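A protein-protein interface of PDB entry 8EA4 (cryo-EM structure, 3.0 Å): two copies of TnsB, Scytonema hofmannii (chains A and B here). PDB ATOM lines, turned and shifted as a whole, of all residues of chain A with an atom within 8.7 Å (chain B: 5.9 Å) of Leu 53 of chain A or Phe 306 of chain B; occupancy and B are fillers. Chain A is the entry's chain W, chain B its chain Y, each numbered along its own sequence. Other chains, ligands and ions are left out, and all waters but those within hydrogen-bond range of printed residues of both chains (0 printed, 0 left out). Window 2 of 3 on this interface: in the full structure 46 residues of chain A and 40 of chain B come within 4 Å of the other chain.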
ATOM      1  N   LEU A  46      -4.557 -12.611 -17.940  1.00  0.00           N
ATOM      2  CA  LEU A  46      -5.353 -12.062 -19.037  1.00  0.00           C
ATOM      3  C   LEU A  46      -5.224 -10.535 -19.140  1.00  0.00           C
ATOM      4  O   LEU A  46      -5.043 -10.022 -20.239  1.00  0.00           O
ATOM      5  CB  LEU A  46      -6.810 -12.512 -18.862  1.00  0.00           C
ATOM      6  CG  LEU A  46      -7.797 -11.899 -19.863  1.00  0.00           C
ATOM      7  CD1 LEU A  46      -7.521 -12.410 -21.273  1.00  0.00           C
ATOM      8  CD2 LEU A  46      -9.217 -12.279 -19.462  1.00  0.00           C
ATOM      9  N   GLU A  47      -5.244  -9.795 -18.033  1.00  0.00           N
ATOM     10  CA  GLU A  47      -5.013  -8.344 -18.078  1.00  0.00           C
ATOM     11  C   GLU A  47      -3.596  -7.999 -18.545  1.00  0.00           C
ATOM     12  O   GLU A  47      -3.399  -7.049 -19.304  1.00  0.00           O
ATOM     13  CB  GLU A  47      -5.219  -7.701 -16.705  1.00  0.00           C
ATOM     14  CG  GLU A  47      -6.667  -7.755 -16.217  1.00  0.00           C
ATOM     15  CD  GLU A  47      -6.849  -7.048 -14.866  1.00  0.00           C
ATOM     16  OE1 GLU A  47      -5.894  -6.447 -14.330  1.00  0.00           O
ATOM     17  OE2 GLU A  47      -7.980  -7.075 -14.341  1.00  0.00           O
ATOM     18  N   VAL A  48      -2.602  -8.777 -18.122  1.00  0.00           N
ATOM     19  CA  VAL A  48      -1.220  -8.615 -18.584  1.00  0.00           C
ATOM     20  C   VAL A  48      -1.114  -8.895 -20.078  1.00  0.00           C
ATOM     21  O   VAL A  48      -0.557  -8.085 -20.811  1.00  0.00           O
ATOM     22  CB  VAL A  48      -0.263  -9.498 -17.770  1.00  0.00           C
ATOM     23  CG1 VAL A  48       1.140  -9.518 -18.369  1.00  0.00           C
ATOM     24  CG2 VAL A  48      -0.175  -8.968 -16.338  1.00  0.00           C
ATOM     25  N   ILE A  49      -1.712  -9.979 -20.564  1.00  0.00           N
ATOM     26  CA  ILE A  49      -1.743 -10.286 -21.989  1.00  0.00           C
ATOM     27  C   ILE A  49      -2.458  -9.192 -22.780  1.00  0.00           C
ATOM     28  O   ILE A  49      -1.932  -8.752 -23.793  1.00  0.00           O
ATOM     29  CB  ILE A  49      -2.341 -11.686 -22.199  1.00  0.00           C
ATOM     30  CG1 ILE A  49      -1.328 -12.782 -21.806  1.00  0.00           C
ATOM     31  CG2 ILE A  49      -2.856 -11.918 -23.623  1.00  0.00           C
ATOM     32  CD1 ILE A  49       0.007 -12.795 -22.565  1.00  0.00           C
ATOM     33  N   GLN A  50      -3.576  -8.658 -22.295  1.00  0.00           N
ATOM     34  CA  GLN A  50      -4.228  -7.510 -22.935  1.00  0.00           C
ATOM     35  C   GLN A  50      -3.329  -6.263 -22.940  1.00  0.00           C
ATOM     36  O   GLN A  50      -3.263  -5.556 -23.942  1.00  0.00           O
ATOM     37  CB  GLN A  50      -5.572  -7.228 -22.254  1.00  0.00           C
ATOM     38  CG  GLN A  50      -6.620  -8.284 -22.637  1.00  0.00           C
ATOM     39  CD  GLN A  50      -7.896  -8.207 -21.810  1.00  0.00           C
ATOM     40  OE1 GLN A  50      -8.074  -7.382 -20.924  1.00  0.00           O
ATOM     41  NE2 GLN A  50      -8.843  -9.077 -22.079  1.00  0.00           N
ATOM     42  N   SER A  51      -2.558  -6.024 -21.875  1.00  0.00           N
ATOM     43  CA  SER A  51      -1.576  -4.924 -21.816  1.00  0.00           C
ATOM     44  C   SER A  51      -0.445  -5.077 -22.838  1.00  0.00           C
ATOM     45  O   SER A  51       0.147  -4.095 -23.264  1.00  0.00           O
ATOM     46  CB  SER A  51      -0.959  -4.823 -20.418  1.00  0.00           C
ATOM     47  OG  SER A  51      -1.962  -4.707 -19.427  1.00  0.00           O
ATOM     48  N   LEU A  52      -0.159  -6.308 -23.254  1.00  0.00           N
ATOM     49  CA  LEU A  52       0.878  -6.665 -24.224  1.00  0.00           C
ATOM     50  C   LEU A  52       0.311  -6.976 -25.623  1.00  0.00           C
ATOM     51  O   LEU A  52       1.055  -7.381 -26.514  1.00  0.00           O
ATOM     52  CB  LEU A  52       1.682  -7.839 -23.638  1.00  0.00           C
ATOM     53  CG  LEU A  52       2.374  -7.503 -22.305  1.00  0.00           C
ATOM     54  CD1 LEU A  52       2.933  -8.769 -21.674  1.00  0.00           C
ATOM     55  CD2 LEU A  52       3.514  -6.508 -22.502  1.00  0.00           C
ATOM     56  N   LEU A  53      -0.993  -6.781 -25.836  1.00  0.00           N
ATOM     57  CA  LEU A  53      -1.669  -7.076 -27.101  1.00  0.00           C
ATOM     58  C   LEU A  53      -1.650  -5.899 -28.090  1.00  0.00           C
ATOM     59  O   LEU A  53      -1.633  -6.103 -29.301  1.00  0.00           O
ATOM     60  CB  LEU A  53      -3.101  -7.529 -26.757  1.00  0.00           C
ATOM     61  CG  LEU A  53      -3.926  -8.091 -27.925  1.00  0.00           C
ATOM     62  CD1 LEU A  53      -3.223  -9.251 -28.626  1.00  0.00           C
ATOM     63  CD2 LEU A  53      -5.249  -8.620 -27.373  1.00  0.00           C
ATOM     64  N   GLU A  54      -1.638  -4.666 -27.577  1.00  0.00           N
ATOM     65  CA  GLU A  54      -1.632  -3.425 -28.363  1.00  0.00           C
ATOM     66  C   GLU A  54      -0.332  -3.096 -29.127  1.00  0.00           C
ATOM     67  O   GLU A  54      -0.422  -2.678 -30.282  1.00  0.00           O
ATOM     68  CB  GLU A  54      -1.992  -2.259 -27.417  1.00  0.00           C
ATOM     69  CG  GLU A  54      -1.668  -0.824 -27.883  1.00  0.00           C
ATOM     70  CD  GLU A  54      -2.162  -0.450 -29.288  1.00  0.00           C
ATOM     71  OE1 GLU A  54      -3.156  -1.035 -29.762  1.00  0.00           O
ATOM     72  OE2 GLU A  54      -1.584   0.477 -29.895  1.00  0.00           O
ATOM     73  N   PRO A  55       0.865  -3.162 -28.512  1.00  0.00           N
ATOM     74  CA  PRO A  55       1.987  -2.332 -28.943  1.00  0.00           C
ATOM     75  C   PRO A  55       2.600  -2.738 -30.285  1.00  0.00           C
ATOM     76  O   PRO A  55       2.519  -3.894 -30.713  1.00  0.00           O
ATOM     77  CB  PRO A  55       2.998  -2.401 -27.800  1.00  0.00           C
ATOM     78  CG  PRO A  55       2.730  -3.771 -27.186  1.00  0.00           C
ATOM     79  CD  PRO A  55       1.217  -3.886 -27.304  1.00  0.00           C
ATOM     80  N   CYS A  56       3.283  -1.773 -30.905  1.00  0.00           N
ATOM     81  CA  CYS A  56       3.983  -1.931 -32.185  1.00  0.00           C
ATOM     82  C   CYS A  56       5.448  -1.433 -32.155  1.00  0.00           C
ATOM     83  O   CYS A  56       6.163  -1.599 -33.142  1.00  0.00           O
ATOM     84  CB  CYS A  56       3.169  -1.215 -33.276  1.00  0.00           C
ATOM     85  SG  CYS A  56       1.455  -1.818 -33.368  1.00  0.00           S
ATOM     86  N   TYR A  61       7.404  -2.280 -26.070  1.00  0.00           N
ATOM     87  CA  TYR A  61       7.421  -3.686 -25.585  1.00  0.00           C
ATOM     88  C   TYR A  61       8.225  -3.721 -24.282  1.00  0.00           C
ATOM     89  O   TYR A  61       7.709  -4.242 -23.275  1.00  0.00           O
ATOM     90  CB  TYR A  61       8.055  -4.617 -26.618  1.00  0.00           C
ATOM     91  CG  TYR A  61       7.305  -4.758 -27.920  1.00  0.00           C
ATOM     92  CD1 TYR A  61       6.296  -5.694 -28.073  1.00  0.00           C
ATOM     93  CD2 TYR A  61       7.615  -3.956 -29.005  1.00  0.00           C
ATOM     94  CE1 TYR A  61       5.611  -5.824 -29.270  1.00  0.00           C
ATOM     95  CE2 TYR A  61       6.941  -4.072 -30.206  1.00  0.00           C
ATOM     96  CZ  TYR A  61       5.935  -5.011 -30.342  1.00  0.00           C
ATOM     97  OH  TYR A  61       5.272  -5.127 -31.539  1.00  0.00           O
ATOM     98  N   LYS A  64       6.283  -2.035 -21.265  1.00  0.00           N
ATOM     99  CA  LYS A  64       5.107  -2.777 -20.787  1.00  0.00           C
ATOM    100  C   LYS A  64       5.453  -4.165 -20.252  1.00  0.00           C
ATOM    101  O   LYS A  64       4.842  -4.589 -19.283  1.00  0.00           O
ATOM    102  CB  LYS A  64       4.031  -2.815 -21.879  1.00  0.00           C
ATOM    103  CG  LYS A  64       3.487  -1.402 -22.136  1.00  0.00           C
ATOM    104  CD  LYS A  64       2.182  -1.420 -22.930  1.00  0.00           C
ATOM    105  CE  LYS A  64       1.654   0.010 -23.060  1.00  0.00           C
ATOM    106  NZ  LYS A  64       0.342   0.061 -23.741  1.00  0.00           N
ATOM    107  N   VAL A  83       4.027 -14.624 -22.358  1.00  0.00           N
ATOM    108  CA  VAL A  83       3.625 -14.202 -23.707  1.00  0.00           C
ATOM    109  C   VAL A  83       3.828 -15.338 -24.701  1.00  0.00           C
ATOM    110  O   VAL A  83       2.929 -15.624 -25.476  1.00  0.00           O
ATOM    111  CB  VAL A  83       4.382 -12.943 -24.161  1.00  0.00           C
ATOM    112  CG1 VAL A  83       4.060 -12.561 -25.613  1.00  0.00           C
ATOM    113  CG2 VAL A  83       4.004 -11.746 -23.288  1.00  0.00           C
ATOM    114  N   TRP A  86       0.989 -17.889 -24.423  1.00  0.00           N
ATOM    115  CA  TRP A  86      -0.193 -17.316 -25.076  1.00  0.00           C
ATOM    116  C   TRP A  86      -0.025 -17.144 -26.601  1.00  0.00           C
ATOM    117  O   TRP A  86      -1.007 -17.076 -27.335  1.00  0.00           O
ATOM    118  CB  TRP A  86      -0.531 -15.994 -24.386  1.00  0.00           C
ATOM    119  CG  TRP A  86      -1.475 -15.133 -25.157  1.00  0.00           C
ATOM    120  CD1 TRP A  86      -2.822 -15.211 -25.131  1.00  0.00           C
ATOM    121  CD2 TRP A  86      -1.148 -14.194 -26.224  1.00  0.00           C
ATOM    122  NE1 TRP A  86      -3.348 -14.363 -26.084  1.00  0.00           N
ATOM    123  CE2 TRP A  86      -2.363 -13.718 -26.792  1.00  0.00           C
ATOM    124  CE3 TRP A  86       0.054 -13.743 -26.807  1.00  0.00           C
ATOM    125  CZ2 TRP A  86      -2.388 -12.824 -27.868  1.00  0.00           C
ATOM    126  CZ3 TRP A  86       0.043 -12.844 -27.889  1.00  0.00           C
ATOM    127  CH2 TRP A  86      -1.174 -12.378 -28.417  1.00  0.00           C
ATOM    128  N   LEU B 256     -19.595 -10.787 -35.210  1.00  0.00           N
ATOM    129  CA  LEU B 256     -18.176 -10.672 -35.469  1.00  0.00           C
ATOM    130  C   LEU B 256     -17.691 -11.892 -36.230  1.00  0.00           C
ATOM    131  O   LEU B 256     -17.054 -11.783 -37.288  1.00  0.00           O
ATOM    132  CB  LEU B 256     -17.401 -10.525 -34.154  1.00  0.00           C
ATOM    133  CG  LEU B 256     -15.875 -10.438 -34.288  1.00  0.00           C
ATOM    134  CD1 LEU B 256     -15.504  -9.196 -35.087  1.00  0.00           C
ATOM    135  CD2 LEU B 256     -15.244 -10.406 -32.904  1.00  0.00           C
ATOM    136  N   ILE B 260     -16.034 -12.025 -39.882  1.00  0.00           N
ATOM    137  CA  ILE B 260     -14.678 -12.494 -40.053  1.00  0.00           C
ATOM    138  C   ILE B 260     -14.536 -13.602 -41.080  1.00  0.00           C
ATOM    139  O   ILE B 260     -13.620 -13.588 -41.895  1.00  0.00           O
ATOM    140  CB  ILE B 260     -14.116 -12.987 -38.707  1.00  0.00           C
ATOM    141  CG1 ILE B 260     -13.884 -11.807 -37.760  1.00  0.00           C
ATOM    142  CG2 ILE B 260     -12.826 -13.764 -38.922  1.00  0.00           C
ATOM    143  CD1 ILE B 260     -13.511 -12.216 -36.354  1.00  0.00           C
ATOM    144  N   LYS B 280      -9.575 -10.356 -40.312  1.00  0.00           N
ATOM    145  CA  LYS B 280      -9.481  -9.825 -38.923  1.00  0.00           C
ATOM    146  C   LYS B 280      -9.325  -8.306 -38.862  1.00  0.00           C
ATOM    147  O   LYS B 280      -8.473  -7.772 -39.592  1.00  0.00           O
ATOM    148  CB  LYS B 280      -8.310 -10.476 -38.186  1.00  0.00           C
ATOM    149  CG  LYS B 280      -8.223 -10.123 -36.709  1.00  0.00           C
ATOM    150  CD  LYS B 280      -7.155 -10.947 -36.003  1.00  0.00           C
ATOM    151  CE  LYS B 280      -5.758 -10.529 -36.435  1.00  0.00           C
ATOM    152  NZ  LYS B 280      -5.395  -9.181 -35.920  1.00  0.00           N
ATOM    153  N   PRO B 281     -10.094  -7.590 -38.013  1.00  0.00           N
ATOM    154  CA  PRO B 281      -9.992  -6.138 -37.921  1.00  0.00           C
ATOM    155  C   PRO B 281      -8.695  -5.828 -37.175  1.00  0.00           C
ATOM    156  O   PRO B 281      -8.214  -6.709 -36.519  1.00  0.00           O
ATOM    157  CB  PRO B 281     -11.162  -5.745 -37.020  1.00  0.00           C
ATOM    158  CG  PRO B 281     -11.445  -6.981 -36.206  1.00  0.00           C
ATOM    159  CD  PRO B 281     -11.179  -8.126 -37.158  1.00  0.00           C
ATOM    160  N   GLU B 282      -8.108  -4.630 -37.260  1.00  0.00           N
ATOM    161  CA  GLU B 282      -7.002  -4.282 -36.348  1.00  0.00           C
ATOM    162  C   GLU B 282      -7.533  -3.886 -34.960  1.00  0.00           C
ATOM    163  O   GLU B 282      -7.003  -4.307 -33.937  1.00  0.00           O
ATOM    164  CB  GLU B 282      -6.098  -3.197 -36.952  1.00  0.00           C
ATOM    165  CG  GLU B 282      -4.791  -3.013 -36.166  1.00  0.00           C
ATOM    166  CD  GLU B 282      -4.135  -1.646 -36.418  1.00  0.00           C
ATOM    167  OE1 GLU B 282      -4.104  -1.198 -37.578  1.00  0.00           O
ATOM    168  OE2 GLU B 282      -3.657  -1.019 -35.445  1.00  0.00           O
ATOM    169  N   HIS B 283      -8.629  -3.175 -34.974  1.00  0.00           N
ATOM    170  CA  HIS B 283      -9.264  -2.941 -33.664  1.00  0.00           C
ATOM    171  C   HIS B 283     -10.741  -3.317 -33.834  1.00  0.00           C
ATOM    172  O   HIS B 283     -11.112  -3.733 -34.932  1.00  0.00           O
ATOM    173  CB  HIS B 283      -9.041  -1.511 -33.168  1.00  0.00           C
ATOM    174  CG  HIS B 283      -7.614  -1.083 -33.055  1.00  0.00           C
ATOM    175  ND1 HIS B 283      -7.154  -0.264 -32.060  1.00  0.00           N
ATOM    176  CD2 HIS B 283      -6.554  -1.380 -33.855  1.00  0.00           C
ATOM    177  CE1 HIS B 283      -5.851  -0.067 -32.229  1.00  0.00           C
ATOM    178  NE2 HIS B 283      -5.458  -0.753 -33.336  1.00  0.00           N
ATOM    179  N   PHE B 284     -11.519  -3.259 -32.765  1.00  0.00           N
ATOM    180  CA  PHE B 284     -12.974  -3.534 -32.861  1.00  0.00           C
ATOM    181  C   PHE B 284     -13.773  -2.680 -31.879  1.00  0.00           C
ATOM    182  O   PHE B 284     -13.590  -2.845 -30.664  1.00  0.00           O
ATOM    183  CB  PHE B 284     -13.250  -5.012 -32.585  1.00  0.00           C
ATOM    184  CG  PHE B 284     -14.691  -5.404 -32.770  1.00  0.00           C
ATOM    185  CD1 PHE B 284     -15.396  -4.994 -33.891  1.00  0.00           C
ATOM    186  CD2 PHE B 284     -15.341  -6.180 -31.823  1.00  0.00           C
ATOM    187  CE1 PHE B 284     -16.720  -5.352 -34.061  1.00  0.00           C
ATOM    188  CE2 PHE B 284     -16.662  -6.541 -31.992  1.00  0.00           C
ATOM    189  CZ  PHE B 284     -17.353  -6.127 -33.112  1.00  0.00           C
ATOM    190  N   LEU B 297     -15.913 -10.509 -24.554  1.00  0.00           N
ATOM    191  CA  LEU B 297     -15.537 -10.030 -25.902  1.00  0.00           C
ATOM    192  C   LEU B 297     -14.031  -9.777 -25.889  1.00  0.00           C
ATOM    193  O   LEU B 297     -13.373 -10.049 -26.911  1.00  0.00           O
ATOM    194  CB  LEU B 297     -16.293  -8.746 -26.275  1.00  0.00           C
ATOM    195  CG  LEU B 297     -16.039  -8.212 -27.690  1.00  0.00           C
ATOM    196  CD1 LEU B 297     -16.409  -9.279 -28.711  1.00  0.00           C
ATOM    197  CD2 LEU B 297     -16.848  -6.943 -27.906  1.00  0.00           C
ATOM    198  N   SER B 298     -13.460  -9.286 -24.785  1.00  0.00           N
ATOM    199  CA  SER B 298     -12.022  -9.024 -24.684  1.00  0.00           C
ATOM    200  C   SER B 298     -11.187 -10.309 -24.705  1.00  0.00           C
ATOM    201  O   SER B 298     -10.077 -10.311 -25.235  1.00  0.00           O
ATOM    202  CB  SER B 298     -11.734  -8.192 -23.432  1.00  0.00           C
ATOM    203  OG  SER B 298     -11.549  -8.993 -22.280  1.00  0.00           O
ATOM    204  N   ILE B 300     -12.217 -12.871 -26.574  1.00  0.00           N
ATOM    205  CA  ILE B 300     -12.242 -13.073 -28.027  1.00  0.00           C
ATOM    206  C   ILE B 300     -11.204 -12.170 -28.701  1.00  0.00           C
ATOM    207  O   ILE B 300     -10.497 -12.668 -29.576  1.00  0.00           O
ATOM    208  CB  ILE B 300     -13.646 -12.877 -28.636  1.00  0.00           C
ATOM    209  CG1 ILE B 300     -14.643 -13.914 -28.095  1.00  0.00           C
ATOM    210  CG2 ILE B 300     -13.578 -12.967 -30.166  1.00  0.00           C
ATOM    211  CD1 ILE B 300     -16.105 -13.590 -28.414  1.00  0.00           C
ATOM    212  N   GLY B 301     -11.014 -10.936 -28.243  1.00  0.00           N
ATOM    213  CA  GLY B 301      -9.954 -10.061 -28.727  1.00  0.00           C
ATOM    214  C   GLY B 301      -8.563 -10.674 -28.561  1.00  0.00           C
ATOM    215  O   GLY B 301      -7.810 -10.775 -29.522  1.00  0.00           O
ATOM    216  N   ALA B 302      -8.227 -11.160 -27.369  1.00  0.00           N
ATOM    217  CA  ALA B 302      -6.926 -11.767 -27.107  1.00  0.00           C
ATOM    218  C   ALA B 302      -6.730 -13.140 -27.778  1.00  0.00           C
ATOM    219  O   ALA B 302      -5.625 -13.455 -28.202  1.00  0.00           O
ATOM    220  CB  ALA B 302      -6.741 -11.861 -25.594  1.00  0.00           C
ATOM    221  N   LEU B 304      -8.048 -14.109 -30.700  1.00  0.00           N
ATOM    222  CA  LEU B 304      -7.939 -13.969 -32.177  1.00  0.00           C
ATOM    223  C   LEU B 304      -6.833 -12.958 -32.499  1.00  0.00           C
ATOM    224  O   LEU B 304      -6.287 -13.021 -33.607  1.00  0.00           O
ATOM    225  CB  LEU B 304      -9.267 -13.508 -32.788  1.00  0.00           C
ATOM    226  CG  LEU B 304     -10.436 -14.493 -32.663  1.00  0.00           C
ATOM    227  CD1 LEU B 304     -11.702 -13.850 -33.211  1.00  0.00           C
ATOM    228  CD2 LEU B 304     -10.104 -15.773 -33.415  1.00  0.00           C
ATOM    229  N   GLY B 305      -6.474 -12.057 -31.585  1.00  0.00           N
ATOM    230  CA  GLY B 305      -5.375 -11.109 -31.734  1.00  0.00           C
ATOM    231  C   GLY B 305      -5.793  -9.739 -32.258  1.00  0.00           C
ATOM    232  O   GLY B 305      -5.184  -9.244 -33.200  1.00  0.00           O
ATOM    233  N   PHE B 306      -6.811  -9.100 -31.687  1.00  0.00           N
ATOM    234  CA  PHE B 306      -7.161  -7.697 -31.968  1.00  0.00           C
ATOM    235  C   PHE B 306      -7.614  -6.966 -30.695  1.00  0.00           C
ATOM    236  O   PHE B 306      -8.047  -7.596 -29.734  1.00  0.00           O
ATOM    237  CB  PHE B 306      -8.218  -7.607 -33.082  1.00  0.00           C
ATOM    238  CG  PHE B 306      -9.586  -8.115 -32.696  1.00  0.00           C
ATOM    239  CD1 PHE B 306     -10.423  -7.325 -31.890  1.00  0.00           C
ATOM    240  CD2 PHE B 306     -10.017  -9.383 -33.113  1.00  0.00           C
ATOM    241  CE1 PHE B 306     -11.640  -7.840 -31.425  1.00  0.00           C
ATOM    242  CE2 PHE B 306     -11.254  -9.879 -32.676  1.00  0.00           C
ATOM    243  CZ  PHE B 306     -12.046  -9.122 -31.800  1.00  0.00           C
ATOM    244  N   VAL B 307      -7.541  -5.635 -30.676  1.00  0.00           N
ATOM    245  CA  VAL B 307      -7.895  -4.838 -29.492  1.00  0.00           C
ATOM    246  C   VAL B 307      -9.366  -4.432 -29.541  1.00  0.00           C
ATOM    247  O   VAL B 307      -9.808  -3.800 -30.499  1.00  0.00           O
ATOM    248  CB  VAL B 307      -6.997  -3.597 -29.363  1.00  0.00           C
ATOM    249  CG1 VAL B 307      -7.356  -2.771 -28.125  1.00  0.00           C
ATOM    250  CG2 VAL B 307      -5.523  -3.976 -29.229  1.00  0.00           C
ATOM    251  N   CYS B 308     -10.129  -4.754 -28.499  1.00  0.00           N
ATOM    252  CA  CYS B 308     -11.493  -4.254 -28.318  1.00  0.00           C
ATOM    253  C   CYS B 308     -11.522  -2.819 -27.776  1.00  0.00           C
ATOM    254  O   CYS B 308     -10.778  -2.485 -26.857  1.00  0.00           O
ATOM    255  CB  CYS B 308     -12.244  -5.153 -27.339  1.00  0.00           C
ATOM    256  SG  CYS B 308     -12.326  -6.840 -27.970  1.00  0.00           S
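The indole nitrogen (NE1) of Trp 86 of chain A sits at hydrogen-bond distance from the backbone carbonyl oxygen (O) of Ala 302 of chain B, at 3.2 Å.
NE2 of Gln 50 of chain A is in hydrogen-bond range of OG of Ser 298 of chain B, 2.7 Å away.
The backbone carbonyl oxygen of Gly 301 of chain B lies within hydrogen-bond range of the backbone NH of Phe 306 of chain B.
OE2 of Glu 282 of chain B lies within hydrogen-bond range of NE2 of His 283 of chain B, at 2.8 Å.
SG of Cys 56 of chain A lies within hydrogen-bond range of O of Glu 54 of chain A (3.7 Å).
The backbone carbonyl oxygen (O) of Val 307 of chain B sits at hydrogen-bond distance from the backbone NH (N) of Phe 284 of chain B, at 2.9 Å.
Leu 53 of chain A touches Gly 301 of chain B.
CA of Ala 302 of chain B touches CD2 of Leu 53 of chain A, at 3.6 Å.
Phe 306 of chain B touches Leu 53 of chain A.
Glu 54 of chain A touches His 283 of chain B (OE1 to CE1, 3.8 Å).
Glu 54 of chain A touches Val 307 of chain B.
Phe 306 of chain B touches one residue of chain A.
Printed residues of chain A within 4 Å of Val 307 of chain B: Glu 54.
Of the printed residues of chain B, Glu 54 of chain A touches His 283 (3.8 Å) and Val 307 (3.8 Å).
Val 48 of chain A touches none of the printed residues of chain B.
The nearest residue of chain A that does not touch Phe 306 of chain B is Trp 86 of chain A (6.9 Å).
The nearest printed residue of chain A that does not touch Ala 302 of chain B is Ile 49 of chain A (4.4 Å).
Of the 17 printed residues of chain B, 6 touch a printed residue of chain A.
Among the printed residues, 7 pairs touch across the chains.
No position is printed for both chains.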
